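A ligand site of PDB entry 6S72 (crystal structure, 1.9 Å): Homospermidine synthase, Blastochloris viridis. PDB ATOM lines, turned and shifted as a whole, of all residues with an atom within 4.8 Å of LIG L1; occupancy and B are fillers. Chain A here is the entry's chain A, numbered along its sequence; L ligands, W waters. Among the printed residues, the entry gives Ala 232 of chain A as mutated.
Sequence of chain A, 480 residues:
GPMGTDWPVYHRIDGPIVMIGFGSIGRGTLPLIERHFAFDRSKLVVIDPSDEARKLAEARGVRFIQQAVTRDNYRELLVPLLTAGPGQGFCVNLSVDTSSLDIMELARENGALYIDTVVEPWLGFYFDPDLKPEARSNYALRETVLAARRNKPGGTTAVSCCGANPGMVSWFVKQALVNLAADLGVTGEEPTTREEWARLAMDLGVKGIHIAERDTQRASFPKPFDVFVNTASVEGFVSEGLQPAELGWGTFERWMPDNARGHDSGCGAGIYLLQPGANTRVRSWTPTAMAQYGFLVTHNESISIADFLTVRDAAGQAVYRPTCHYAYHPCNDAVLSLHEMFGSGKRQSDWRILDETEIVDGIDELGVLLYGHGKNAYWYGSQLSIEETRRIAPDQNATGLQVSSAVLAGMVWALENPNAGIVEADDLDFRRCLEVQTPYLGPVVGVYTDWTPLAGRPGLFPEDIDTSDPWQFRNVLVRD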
ATOM      1  N   ILE A  20     -36.262  -1.804  29.966  1.00  0.00           N
ATOM      2  CA  ILE A  20     -35.324  -1.657  31.072  1.00  0.00           C
ATOM      3  C   ILE A  20     -34.126  -0.906  30.518  1.00  0.00           C
ATOM      4  O   ILE A  20     -33.382  -1.431  29.689  1.00  0.00           O
ATOM      5  CB  ILE A  20     -34.925  -3.016  31.641  1.00  0.00           C
ATOM      6  CG1 ILE A  20     -36.187  -3.811  32.009  1.00  0.00           C
ATOM      7  CG2 ILE A  20     -34.035  -2.832  32.854  1.00  0.00           C
ATOM      8  CD1 ILE A  20     -35.886  -5.138  32.652  1.00  0.00           C
ATOM      9  N   GLY A  21     -33.938   0.330  30.969  1.00  0.00           N
ATOM     10  CA  GLY A  21     -32.829   1.130  30.497  1.00  0.00           C
ATOM     11  C   GLY A  21     -33.238   2.063  29.381  1.00  0.00           C
ATOM     12  O   GLY A  21     -33.869   1.645  28.403  1.00  0.00           O
ATOM     13  N   PHE A  22     -32.888   3.344  29.528  1.00  0.00           N
ATOM     14  CA  PHE A  22     -33.244   4.343  28.553  1.00  0.00           C
ATOM     15  C   PHE A  22     -32.009   5.239  28.322  1.00  0.00           C
ATOM     16  O   PHE A  22     -32.038   6.440  28.498  1.00  0.00           O
ATOM     17  CB  PHE A  22     -34.451   5.152  29.021  1.00  0.00           C
ATOM     18  CG  PHE A  22     -35.197   5.835  27.919  1.00  0.00           C
ATOM     19  CD1 PHE A  22     -35.756   5.099  26.886  1.00  0.00           C
ATOM     20  CD2 PHE A  22     -35.373   7.211  27.916  1.00  0.00           C
ATOM     21  CE1 PHE A  22     -36.450   5.726  25.854  1.00  0.00           C
ATOM     22  CE2 PHE A  22     -36.066   7.842  26.898  1.00  0.00           C
ATOM     23  CZ  PHE A  22     -36.604   7.094  25.869  1.00  0.00           C
ATOM     24  N   GLY A  23     -30.912   4.605  27.930  1.00  0.00           N
ATOM     25  CA  GLY A  23     -29.710   5.286  27.498  1.00  0.00           C
ATOM     26  C   GLY A  23     -29.731   5.537  25.999  1.00  0.00           C
ATOM     27  O   GLY A  23     -30.799   5.684  25.393  1.00  0.00           O
ATOM     28  N   SER A  24     -28.547   5.540  25.387  1.00  0.00           N
ATOM     29  CA  SER A  24     -28.487   5.869  23.957  1.00  0.00           C
ATOM     30  C   SER A  24     -29.278   4.874  23.118  1.00  0.00           C
ATOM     31  O   SER A  24     -29.967   5.265  22.162  1.00  0.00           O
ATOM     32  CB  SER A  24     -27.029   5.966  23.493  1.00  0.00           C
ATOM     33  OG  SER A  24     -26.457   4.745  23.080  1.00  0.00           O
ATOM     34  N   ILE A  25     -29.245   3.588  23.467  1.00  0.00           N
ATOM     35  CA  ILE A  25     -29.926   2.604  22.629  1.00  0.00           C
ATOM     36  C   ILE A  25     -31.430   2.613  22.891  1.00  0.00           C
ATOM     37  O   ILE A  25     -32.243   2.503  21.965  1.00  0.00           O
ATOM     38  CB  ILE A  25     -29.335   1.200  22.827  1.00  0.00           C
ATOM     39  CG1 ILE A  25     -27.844   1.198  22.480  1.00  0.00           C
ATOM     40  CG2 ILE A  25     -30.077   0.192  21.947  1.00  0.00           C
ATOM     41  CD1 ILE A  25     -27.505   1.804  21.119  1.00  0.00           C
ATOM     42  N   GLY A  26     -31.829   2.748  24.165  1.00  0.00           N
ATOM     43  CA  GLY A  26     -33.243   2.840  24.464  1.00  0.00           C
ATOM     44  C   GLY A  26     -33.903   4.037  23.815  1.00  0.00           C
ATOM     45  O   GLY A  26     -35.025   3.949  23.308  1.00  0.00           O
ATOM     46  N   ARG A  27     -33.196   5.168  23.790  1.00  0.00           N
ATOM     47  CA  ARG A  27     -33.744   6.386  23.192  1.00  0.00           C
ATOM     48  C   ARG A  27     -33.902   6.263  21.686  1.00  0.00           C
ATOM     49  O   ARG A  27     -34.774   6.910  21.101  1.00  0.00           O
ATOM     50  CB  ARG A  27     -32.838   7.574  23.532  1.00  0.00           C
ATOM     51  CG  ARG A  27     -32.834   7.913  25.002  1.00  0.00           C
ATOM     52  CD  ARG A  27     -31.642   8.735  25.436  1.00  0.00           C
ATOM     53  NE  ARG A  27     -31.413   8.557  26.874  1.00  0.00           N
ATOM     54  CZ  ARG A  27     -30.591   9.286  27.618  1.00  0.00           C
ATOM     55  NH1 ARG A  27     -29.896  10.278  27.073  1.00  0.00           N
ATOM     56  NH2 ARG A  27     -30.475   9.033  28.913  1.00  0.00           N
ATOM     57  N   ILE A  47     -38.032   1.861  32.693  1.00  0.00           N
ATOM     58  CA  ILE A  47     -37.417   1.784  34.012  1.00  0.00           C
ATOM     59  C   ILE A  47     -35.954   2.196  33.887  1.00  0.00           C
ATOM     60  O   ILE A  47     -35.197   1.583  33.127  1.00  0.00           O
ATOM     61  CB  ILE A  47     -37.506   0.375  34.617  1.00  0.00           C
ATOM     62  CG1 ILE A  47     -38.915  -0.198  34.453  1.00  0.00           C
ATOM     63  CG2 ILE A  47     -37.078   0.388  36.096  1.00  0.00           C
ATOM     64  CD1 ILE A  47     -39.027  -1.622  34.929  1.00  0.00           C
ATOM     65  N   ASP A  48     -35.546   3.216  34.650  1.00  0.00           N
ATOM     66  CA  ASP A  48     -34.162   3.665  34.589  1.00  0.00           C
ATOM     67  C   ASP A  48     -33.869   4.491  35.828  1.00  0.00           C
ATOM     68  O   ASP A  48     -34.718   5.297  36.207  1.00  0.00           O
ATOM     69  CB  ASP A  48     -33.903   4.486  33.310  1.00  0.00           C
ATOM     70  CG  ASP A  48     -32.422   4.781  33.084  1.00  0.00           C
ATOM     71  OD1 ASP A  48     -31.786   5.421  33.946  1.00  0.00           O
ATOM     72  OD2 ASP A  48     -31.895   4.379  32.021  1.00  0.00           O
ATOM     73  N   PRO A  49     -32.710   4.332  36.459  1.00  0.00           N
ATOM     74  CA  PRO A  49     -32.456   5.086  37.710  1.00  0.00           C
ATOM     75  C   PRO A  49     -32.138   6.562  37.497  1.00  0.00           C
ATOM     76  O   PRO A  49     -32.191   7.312  38.478  1.00  0.00           O
ATOM     77  CB  PRO A  49     -31.262   4.354  38.332  1.00  0.00           C
ATOM     78  CG  PRO A  49     -30.525   3.783  37.161  1.00  0.00           C
ATOM     79  CD  PRO A  49     -31.607   3.391  36.153  1.00  0.00           C
ATOM     80  N   SER A  50     -31.844   7.018  36.286  1.00  0.00           N
ATOM     81  CA  SER A  50     -31.282   8.350  36.118  1.00  0.00           C
ATOM     82  C   SER A  50     -32.340   9.416  35.885  1.00  0.00           C
ATOM     83  O   SER A  50     -33.355   9.178  35.226  1.00  0.00           O
ATOM     84  CB  SER A  50     -30.282   8.372  34.956  1.00  0.00           C
ATOM     85  OG  SER A  50     -30.957   8.647  33.733  1.00  0.00           O
ATOM     86  N   GLN A  67     -36.009   3.605  38.964  1.00  0.00           N
ATOM     87  CA  GLN A  67     -35.436   2.579  39.809  1.00  0.00           C
ATOM     88  C   GLN A  67     -34.277   1.922  39.070  1.00  0.00           C
ATOM     89  O   GLN A  67     -34.327   1.739  37.853  1.00  0.00           O
ATOM     90  CB  GLN A  67     -36.475   1.514  40.185  1.00  0.00           C
ATOM     91  CG  GLN A  67     -37.505   1.985  41.197  1.00  0.00           C
ATOM     92  CD  GLN A  67     -36.911   2.200  42.578  1.00  0.00           C
ATOM     93  OE1 GLN A  67     -35.857   1.649  42.892  1.00  0.00           O
ATOM     94  NE2 GLN A  67     -37.569   3.007  43.395  1.00  0.00           N
ATOM     95  N   ALA A  68     -33.224   1.598  39.814  1.00  0.00           N
ATOM     96  CA  ALA A  68     -32.226   0.657  39.345  1.00  0.00           C
ATOM     97  C   ALA A  68     -32.754  -0.749  39.598  1.00  0.00           C
ATOM     98  O   ALA A  68     -33.152  -1.073  40.719  1.00  0.00           O
ATOM     99  CB  ALA A  68     -30.899   0.869  40.059  1.00  0.00           C
ATOM    100  N   VAL A  69     -32.802  -1.568  38.554  1.00  0.00           N
ATOM    101  CA  VAL A  69     -33.132  -2.982  38.731  1.00  0.00           C
ATOM    102  C   VAL A  69     -31.928  -3.687  39.343  1.00  0.00           C
ATOM    103  O   VAL A  69     -30.822  -3.608  38.804  1.00  0.00           O
ATOM    104  CB  VAL A  69     -33.530  -3.628  37.392  1.00  0.00           C
ATOM    105  CG1 VAL A  69     -33.809  -5.122  37.574  1.00  0.00           C
ATOM    106  CG2 VAL A  69     -34.753  -2.927  36.811  1.00  0.00           C
ATOM    107  N   LEU A  94     -32.277  -3.038  27.623  1.00  0.00           N
ATOM    108  CA  LEU A  94     -31.230  -2.227  27.035  1.00  0.00           C
ATOM    109  C   LEU A  94     -30.470  -1.493  28.117  1.00  0.00           C
ATOM    110  O   LEU A  94     -30.215  -0.292  28.040  1.00  0.00           O
ATOM    111  CB  LEU A  94     -31.827  -1.254  26.022  1.00  0.00           C
ATOM    112  CG  LEU A  94     -32.679  -1.887  24.914  1.00  0.00           C
ATOM    113  CD1 LEU A  94     -33.362  -0.814  24.107  1.00  0.00           C
ATOM    114  CD2 LEU A  94     -31.791  -2.782  24.071  1.00  0.00           C
ATOM    115  N   SER A  95     -30.105  -2.217  29.168  1.00  0.00           N
ATOM    116  CA  SER A  95     -29.551  -1.626  30.364  1.00  0.00           C
ATOM    117  C   SER A  95     -28.092  -2.000  30.540  1.00  0.00           C
ATOM    118  O   SER A  95     -27.531  -2.821  29.797  1.00  0.00           O
ATOM    119  CB  SER A  95     -30.364  -2.079  31.592  1.00  0.00           C
ATOM    120  OG  SER A  95     -30.336  -3.490  31.715  1.00  0.00           O
ATOM    121  N   VAL A  96     -27.453  -1.358  31.514  1.00  0.00           N
ATOM    122  CA  VAL A  96     -26.203  -1.831  32.081  1.00  0.00           C
ATOM    123  C   VAL A  96     -26.491  -2.274  33.519  1.00  0.00           C
ATOM    124  O   VAL A  96     -27.530  -1.940  34.099  1.00  0.00           O
ATOM    125  CB  VAL A  96     -25.085  -0.781  32.038  1.00  0.00           C
ATOM    126  CG1 VAL A  96     -24.716  -0.404  30.599  1.00  0.00           C
ATOM    127  CG2 VAL A  96     -25.478   0.450  32.850  1.00  0.00           C
ATOM    128  N   ASP A  97     -25.548  -3.018  34.099  1.00  0.00           N
ATOM    129  CA  ASP A  97     -25.518  -3.341  35.518  1.00  0.00           C
ATOM    130  C   ASP A  97     -26.586  -4.344  35.948  1.00  0.00           C
ATOM    131  O   ASP A  97     -26.732  -4.588  37.155  1.00  0.00           O
ATOM    132  CB  ASP A  97     -25.649  -2.080  36.380  1.00  0.00           C
ATOM    133  CG  ASP A  97     -24.431  -1.182  36.284  1.00  0.00           C
ATOM    134  OD1 ASP A  97     -23.433  -1.584  35.639  1.00  0.00           O
ATOM    135  OD2 ASP A  97     -24.469  -0.072  36.860  1.00  0.00           O
ATOM    136  N   THR A  98     -27.294  -4.959  35.011  1.00  0.00           N
ATOM    137  CA  THR A  98     -28.336  -5.922  35.314  1.00  0.00           C
ATOM    138  C   THR A  98     -27.976  -7.284  34.730  1.00  0.00           C
ATOM    139  O   THR A  98     -27.240  -7.391  33.746  1.00  0.00           O
ATOM    140  CB  THR A  98     -29.676  -5.474  34.727  1.00  0.00           C
ATOM    141  OG1 THR A  98     -29.544  -5.359  33.303  1.00  0.00           O
ATOM    142  CG2 THR A  98     -30.087  -4.135  35.291  1.00  0.00           C
ATOM    143  N   THR A 117     -29.180  -7.022  24.192  1.00  0.00           N
ATOM    144  CA  THR A 117     -28.086  -6.830  23.252  1.00  0.00           C
ATOM    145  C   THR A 117     -26.736  -7.242  23.834  1.00  0.00           C
ATOM    146  O   THR A 117     -25.694  -6.910  23.251  1.00  0.00           O
ATOM    147  CB  THR A 117     -28.003  -5.369  22.817  1.00  0.00           C
ATOM    148  OG1 THR A 117     -27.673  -4.558  23.948  1.00  0.00           O
ATOM    149  CG2 THR A 117     -29.304  -4.930  22.202  1.00  0.00           C
ATOM    150  N   VAL A 118     -26.719  -7.920  24.973  1.00  0.00           N
ATOM    151  CA  VAL A 118     -25.497  -8.256  25.672  1.00  0.00           C
ATOM    152  C   VAL A 118     -25.878  -9.211  26.791  1.00  0.00           C
ATOM    153  O   VAL A 118     -26.996  -9.148  27.311  1.00  0.00           O
ATOM    154  CB  VAL A 118     -24.807  -6.990  26.223  1.00  0.00           C
ATOM    155  CG1 VAL A 118     -25.763  -6.198  27.119  1.00  0.00           C
ATOM    156  CG2 VAL A 118     -23.543  -7.370  26.967  1.00  0.00           C
ATOM    157  N   GLU A 120     -25.261  -9.298  30.124  1.00  0.00           N
ATOM    158  CA  GLU A 120     -24.753  -8.441  31.183  1.00  0.00           C
ATOM    159  C   GLU A 120     -24.881  -9.144  32.536  1.00  0.00           C
ATOM    160  O   GLU A 120     -25.837  -9.898  32.749  1.00  0.00           O
ATOM    161  CB  GLU A 120     -25.527  -7.121  31.206  1.00  0.00           C
ATOM    162  CG  GLU A 120     -25.062  -6.105  32.231  1.00  0.00           C
ATOM    163  CD  GLU A 120     -23.852  -5.307  31.788  1.00  0.00           C
ATOM    164  OE1 GLU A 120     -23.213  -5.702  30.781  1.00  0.00           O
ATOM    165  OE2 GLU A 120     -23.525  -4.294  32.451  1.00  0.00           O
ATOM    166  N   GLY A 163     -28.223  -7.013  19.044  1.00  0.00           N
ATOM    167  CA  GLY A 163     -27.948  -5.648  18.646  1.00  0.00           C
ATOM    168  C   GLY A 163     -27.253  -5.592  17.298  1.00  0.00           C
ATOM    169  O   GLY A 163     -27.505  -6.446  16.443  1.00  0.00           O
ATOM    170  N   ALA A 164     -26.369  -4.611  17.075  1.00  0.00           N
ATOM    171  CA  ALA A 164     -25.611  -4.570  15.829  1.00  0.00           C
ATOM    172  C   ALA A 164     -24.489  -5.609  15.819  1.00  0.00           C
ATOM    173  O   ALA A 164     -24.288  -6.304  14.815  1.00  0.00           O
ATOM    174  CB  ALA A 164     -25.011  -3.176  15.623  1.00  0.00           C
ATOM    175  N   ASN A 165     -23.760  -5.715  16.920  1.00  0.00           N
ATOM    176  CA  ASN A 165     -22.705  -6.698  17.072  1.00  0.00           C
ATOM    177  C   ASN A 165     -22.424  -6.857  18.562  1.00  0.00           C
ATOM    178  O   ASN A 165     -21.828  -5.962  19.171  1.00  0.00           O
ATOM    179  CB  ASN A 165     -21.449  -6.286  16.276  1.00  0.00           C
ATOM    180  CG  ASN A 165     -20.956  -4.879  16.601  1.00  0.00           C
ATOM    181  OD1 ASN A 165     -21.715  -3.907  16.657  1.00  0.00           O
ATOM    182  ND2 ASN A 165     -19.652  -4.772  16.790  1.00  0.00           N
ATOM    183  N   PRO A 166     -22.846  -7.959  19.201  1.00  0.00           N
ATOM    184  CA  PRO A 166     -23.549  -9.118  18.613  1.00  0.00           C
ATOM    185  C   PRO A 166     -24.927  -8.768  18.070  1.00  0.00           C
ATOM    186  O   PRO A 166     -25.547  -7.779  18.506  1.00  0.00           O
ATOM    187  CB  PRO A 166     -23.668 -10.106  19.775  1.00  0.00           C
ATOM    188  CG  PRO A 166     -23.646  -9.243  21.007  1.00  0.00           C
ATOM    189  CD  PRO A 166     -22.737  -8.075  20.673  1.00  0.00           C
ATOM    190  N   ALA A 232     -21.549   5.189  21.532  1.00  0.00           N
ATOM    191  CA  ALA A 232     -22.532   4.417  22.292  1.00  0.00           C
ATOM    192  C   ALA A 232     -21.994   4.292  23.712  1.00  0.00           C
ATOM    193  O   ALA A 232     -20.981   4.887  24.065  1.00  0.00           O
ATOM    194  CB  ALA A 232     -22.814   3.056  21.639  1.00  0.00           C
ATOM    195  N   SER A 233     -22.694   3.498  24.518  1.00  0.00           N
ATOM    196  CA  SER A 233     -22.386   3.343  25.931  1.00  0.00           C
ATOM    197  C   SER A 233     -20.899   3.437  26.241  1.00  0.00           C
ATOM    198  O   SER A 233     -20.092   2.636  25.756  1.00  0.00           O
ATOM    199  CB  SER A 233     -22.908   2.013  26.465  1.00  0.00           C
ATOM    200  OG  SER A 233     -22.831   1.967  27.882  1.00  0.00           O
ATOM    201  N   GLY A 236     -20.544   0.556  29.089  1.00  0.00           N
ATOM    202  CA  GLY A 236     -20.514  -0.777  28.517  1.00  0.00           C
ATOM    203  C   GLY A 236     -19.251  -1.041  27.719  1.00  0.00           C
ATOM    204  O   GLY A 236     -18.697  -2.143  27.774  1.00  0.00           O
ATOM    205  N   TRP A 351     -17.614  11.341  31.282  1.00  0.00           N
ATOM    206  CA  TRP A 351     -17.762  10.753  29.963  1.00  0.00           C
ATOM    207  C   TRP A 351     -18.957  11.358  29.257  1.00  0.00           C
ATOM    208  O   TRP A 351     -19.848  11.945  29.887  1.00  0.00           O
ATOM    209  CB  TRP A 351     -17.924   9.231  30.016  1.00  0.00           C
ATOM    210  CG  TRP A 351     -19.067   8.723  30.873  1.00  0.00           C
ATOM    211  CD1 TRP A 351     -18.968   8.291  32.172  1.00  0.00           C
ATOM    212  CD2 TRP A 351     -20.445   8.540  30.496  1.00  0.00           C
ATOM    213  NE1 TRP A 351     -20.203   7.851  32.609  1.00  0.00           N
ATOM    214  CE2 TRP A 351     -21.121   8.001  31.601  1.00  0.00           C
ATOM    215  CE3 TRP A 351     -21.168   8.784  29.315  1.00  0.00           C
ATOM    216  CZ2 TRP A 351     -22.489   7.704  31.579  1.00  0.00           C
ATOM    217  CZ3 TRP A 351     -22.526   8.482  29.302  1.00  0.00           C
ATOM    218  CH2 TRP A 351     -23.171   7.953  30.433  1.00  0.00           C
ATOM    219  N   ILE A 353     -21.525  10.543  25.543  1.00  0.00           N
ATOM    220  CA  ILE A 353     -21.880   9.890  24.289  1.00  0.00           C
ATOM    221  C   ILE A 353     -22.247  10.983  23.303  1.00  0.00           C
ATOM    222  O   ILE A 353     -23.039  11.878  23.612  1.00  0.00           O
ATOM    223  CB  ILE A 353     -23.024   8.888  24.488  1.00  0.00           C
ATOM    224  CG1 ILE A 353     -22.607   7.819  25.494  1.00  0.00           C
ATOM    225  CG2 ILE A 353     -23.432   8.296  23.154  1.00  0.00           C
ATOM    226  CD1 ILE A 353     -23.755   6.947  25.978  1.00  0.00           C
ATOM    227  N   VAL A 403     -27.883  -0.537  15.953  1.00  0.00           N
ATOM    228  CA  VAL A 403     -28.264  -1.344  17.109  1.00  0.00           C
ATOM    229  C   VAL A 403     -29.781  -1.354  17.274  1.00  0.00           C
ATOM    230  O   VAL A 403     -30.395  -2.418  17.416  1.00  0.00           O
ATOM    231  CB  VAL A 403     -27.567  -0.835  18.384  1.00  0.00           C
ATOM    232  CG1 VAL A 403     -27.997  -1.691  19.574  1.00  0.00           C
ATOM    233  CG2 VAL A 403     -26.061  -0.812  18.216  1.00  0.00           C
HETATM  234  P1  LIG L   1     -26.020   3.866  28.024  1.00  0.00           P
HETATM  235  O1  LIG L   1     -26.222   4.905  27.218  1.00  0.00           O
HETATM  236  O2  LIG L   1     -24.956   3.799  28.902  1.00  0.00           O
HETATM  237  O3  LIG L   1     -27.255   3.706  28.917  1.00  0.00           O
HETATM  238  C1  LIG L   1     -27.399   2.820  29.961  1.00  0.00           C
HETATM  239  C2  LIG L   1     -28.640   3.026  30.786  1.00  0.00           C
HETATM  240  O4  LIG L   1     -28.845   2.039  31.762  1.00  0.00           O
HETATM  241  C3  LIG L   1     -28.535   4.329  31.561  1.00  0.00           C
HETATM  242  O5  LIG L   1     -29.546   5.127  31.076  1.00  0.00           O
HETATM  243  C4  LIG L   1     -28.603   3.929  33.024  1.00  0.00           C
HETATM  244  O6  LIG L   1     -29.193   4.875  33.805  1.00  0.00           O
HETATM  245  C5  LIG L   1     -29.300   2.596  32.963  1.00  0.00           C
HETATM  246  N1  LIG L   1     -29.090   1.765  34.144  1.00  0.00           N
HETATM  247  C6  LIG L   1     -28.041   1.731  34.883  1.00  0.00           C
HETATM  248  N2  LIG L   1     -28.186   0.871  35.873  1.00  0.00           N
HETATM  249  C7  LIG L   1     -29.323   0.332  35.751  1.00  0.00           C
HETATM  250  C8  LIG L   1     -30.124  -0.626  36.482  1.00  0.00           C
HETATM  251  N3  LIG L   1     -29.621  -1.201  37.544  1.00  0.00           N
HETATM  252  N4  LIG L   1     -31.315  -0.863  36.007  1.00  0.00           N
HETATM  253  C9  LIG L   1     -31.808  -0.278  34.948  1.00  0.00           C
HETATM  254  N5  LIG L   1     -31.145   0.563  34.276  1.00  0.00           N
HETATM  255  C10 LIG L   1     -29.940   0.918  34.597  1.00  0.00           C
HETATM  256  O7  LIG L   1     -25.945   2.551  27.249  1.00  0.00           O
HETATM  257  P2  LIG L   1     -26.468   2.207  25.814  1.00  0.00           P
HETATM  258  O8  LIG L   1     -27.725   2.562  25.724  1.00  0.00           O
HETATM  259  O9  LIG L   1     -25.627   2.733  24.898  1.00  0.00           O
HETATM  260  O10 LIG L   1     -26.305   0.695  25.685  1.00  0.00           O
HETATM  261  C11 LIG L   1     -27.119  -0.170  26.361  1.00  0.00           C
HETATM  262  C12 LIG L   1     -26.683  -1.601  26.362  1.00  0.00           C
HETATM  263  O11 LIG L   1     -26.570  -2.110  25.084  1.00  0.00           O
HETATM  264  C13 LIG L   1     -25.352  -1.762  27.065  1.00  0.00           C
HETATM  265  O12 LIG L   1     -25.348  -2.838  27.948  1.00  0.00           O
HETATM  266  C14 LIG L   1     -24.440  -1.982  25.878  1.00  0.00           C
HETATM  267  O13 LIG L   1     -23.352  -2.755  26.240  1.00  0.00           O
HETATM  268  C15 LIG L   1     -25.330  -2.646  24.856  1.00  0.00           C
HETATM  269  N6  LIG L   1     -24.957  -2.433  23.483  1.00  0.00           N
HETATM  270  C16 LIG L   1     -24.959  -3.397  22.601  1.00  0.00           C
HETATM  271  C17 LIG L   1     -24.624  -3.214  21.314  1.00  0.00           C
HETATM  272  C18 LIG L   1     -24.689  -4.303  20.275  1.00  0.00           C
HETATM  273  O14 LIG L   1     -24.500  -4.038  19.187  1.00  0.00           O
HETATM  274  N7  LIG L   1     -25.027  -5.499  20.622  1.00  0.00           N
HETATM  275  C19 LIG L   1     -24.257  -1.973  20.942  1.00  0.00           C
HETATM  276  C20 LIG L   1     -24.255  -0.960  21.859  1.00  0.00           C
HETATM  277  C21 LIG L   1     -24.629  -1.232  23.126  1.00  0.00           C
HETATM  278  N1  LG2 L   2     -21.079  -1.148  16.493  1.00  0.00           N
HETATM  279  C1  LG2 L   2     -21.257  -0.377  17.709  1.00  0.00           C
HETATM  280  C2  LG2 L   2     -20.966  -1.256  18.921  1.00  0.00           C
HETATM  281  C3  LG2 L   2     -20.514  -0.420  20.116  1.00  0.00           C
HETATM  282  C4  LG2 L   2     -19.877  -1.297  21.185  1.00  0.00           C
HETATM  283  N2  LG2 L   2     -18.452  -1.425  20.914  1.00  0.00           N
HETATM  284  O   HOH W   1     -22.381   5.145  29.232  1.00  0.00           O
HETATM  285  O   HOH W   2     -22.539  -3.685  29.041  1.00  0.00           O
HETATM  286  O   HOH W   3     -30.349   2.245  26.651  1.00  0.00           O
HETATM  287  O   HOH W   4     -29.374   7.961  31.593  1.00  0.00           O
HETATM  288  O   HOH W   5     -21.205  -1.497  24.668  1.00  0.00           O
HETATM  289  O   HOH W   6     -24.885   2.940  35.175  1.00  0.00           O
HETATM  290  O   HOH W   7     -26.856   7.606  27.831  1.00  0.00           O
HETATM  291  O   HOH W   8     -28.008  -3.657  39.292  1.00  0.00           O
HETATM  292  O   HOH W   9     -27.522  -1.047  39.859  1.00  0.00           O
HETATM  293  O   HOH W  10     -21.721  -4.232  21.347  1.00  0.00           O
HETATM  294  O   HOH W  11     -27.394   5.891  35.732  1.00  0.00           O
HETATM  295  O   HOH W  12     -24.921   4.327  31.647  1.00  0.00           O
HETATM  296  O   HOH W  13     -26.546   0.556  38.034  1.00  0.00           O
HETATM  297  O   HOH W  14     -21.733  -4.750  24.171  1.00  0.00           O
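An oxygen (O9) of LIG L1 sits at hydrogen-bond distance from the side-chain hydroxyl (OG) of Ser 24. The backbone NH of Asn 165 is in hydrogen-bond range of an oxygen (O14) of LIG L1 (2.9 Å). O8 of LIG L1 sits at hydrogen-bond distance from N of Ile 25. The backbone NH (N) of Gly 23 is in hydrogen-bond range of an oxygen (O5) of LIG L1 (3.5 Å). The backbone NH (N) of Val 69 is in hydrogen-bond range of a nitrogen (N4) of LIG L1, 3.0 Å away. O of Ser 95 sits at hydrogen-bond distance from O12 of LIG L1. The backbone NH (N) of Ala 164 is in hydrogen-bond range of an oxygen (O14) of LIG L1 (2.9 Å). The side-chain hydroxyl (OG1) of Thr 117 sits at hydrogen-bond distance from an oxygen (O11) of LIG L1, 2.9 Å away. The side-chain carboxylate (OD2) of Asp 48 lies within hydrogen-bond range of an oxygen (O5) of LIG L1 (2.6 Å). The backbone carbonyl oxygen (O) of Val 69 is in hydrogen-bond range of a nitrogen (N3) of LIG L1, at 3.0 Å. The backbone NH (N) of Ser 233 is in hydrogen-bond range of an oxygen (O9) of LIG L1. A nitrogen (N7) of LIG L1 lies within hydrogen-bond range of the backbone carbonyl oxygen (O) of Thr 117. O of Pro 166 is in hydrogen-bond range of N7 of LIG L1. OD1 of Asn 165 lies within hydrogen-bond range of N1 of LG2 L2, 2.8 Å away. An oxygen (O1) of LIG L1 sits at hydrogen-bond distance from the backbone NH of Ser 24. OG of Ser 233 sits at hydrogen-bond distance from O2 of LIG L1 (3.0 Å).
The backbone NH of Leu 94 sits at hydrogen-bond distance from the backbone carbonyl oxygen of Ile 20 (2.8 Å). NE of Arg 27 is in hydrogen-bond range of O of Phe 22 (2.7 Å). O of Ile 20 is in hydrogen-bond range of N of Ser 95, 3.4 Å away. O of Gly 23 lies close to NE of Arg 27, 3.3 Å away. O of Asp 48 is in hydrogen-bond range of N of Gln 67, at 3.5 Å. The side-chain hydroxyl of Ser 233 lies within hydrogen-bond range of the backbone NH of Gly 236. N of Asp 97 sits at hydrogen-bond distance from OE2 of Glu 120 (2.9 Å). The side-chain hydroxyl (OG) of Ser 95 is in hydrogen-bond range of the side-chain hydroxyl (OG1) of Thr 98.
The backbone carbonyl oxygen (O) of Val 96 sits close to a nitrogen (N2) of LIG L1 (3.4 Å). Residues that only touch LIG L1: Ile 20 (3.98 Å), Phe 22 (3.7 Å), Pro 49 (3.4 Å), Ser 50 (3.8 Å), Ala 68 (3.5 Å), Leu 94 (3.5 Å), Asp 97 (3.9 Å), Thr 98 (3.6 Å), Val 118 (3.5 Å), Gly 163 (3.5 Å), Ile 353 (3.4 Å) and Val 403 (3.5 Å). Hydrophobic or aromatic side chains that line LIG L1: Ile 20, Ile 25, Pro 49, Ala 68, Val 69, Val 96, Val 118, Ala 164, Pro 166, Ile 353 and Val 403. 24 residues have an atom within 4 Å of LIG L1: Ile 20, Phe 22, Gly 23, Ser 24, Ile 25, Asp 48, Pro 49, Ser 50, Ala 68, Val 69, Leu 94, Ser 95, Val 96, Asp 97, Thr 98, Thr 117, Val 118, Gly 163, Ala 164, Asn 165, Pro 166, Ser 233, Ile 353 and Val 403.
Water W13 bridges the side-chain carboxylate (OD2) of Asp 97 (2.5 Å) and a nitrogen (N2) of LIG L1 (2.7 Å). Water W3 lies within hydrogen-bond range of the backbone NH of Gly 23 (2.7 Å), an oxygen (O8) of LIG L1 (2.8 Å), the backbone carbonyl oxygen of Leu 94 (2.9 Å) and the backbone NH of Gly 26 (2.9 Å). Water W4 lies within hydrogen-bond range of the side-chain hydroxyl of Ser 50 (2.7 Å), an oxygen (O5) of LIG L1 (2.9 Å) and the guanidinium group of Arg 27 (3.1 Å). Water W1 lies within hydrogen-bond range of O2 of LIG L1 (2.9 Å) and OG of Ser 233 (3.5 Å). Water W2 bridges OE1 of Glu 120 and O13 of LIG L1. Water W8 lies within hydrogen-bond range of O of Asp 97 (2.7 Å), O of Val 69 (2.9 Å) and N3 of LIG L1 (3.4 Å).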
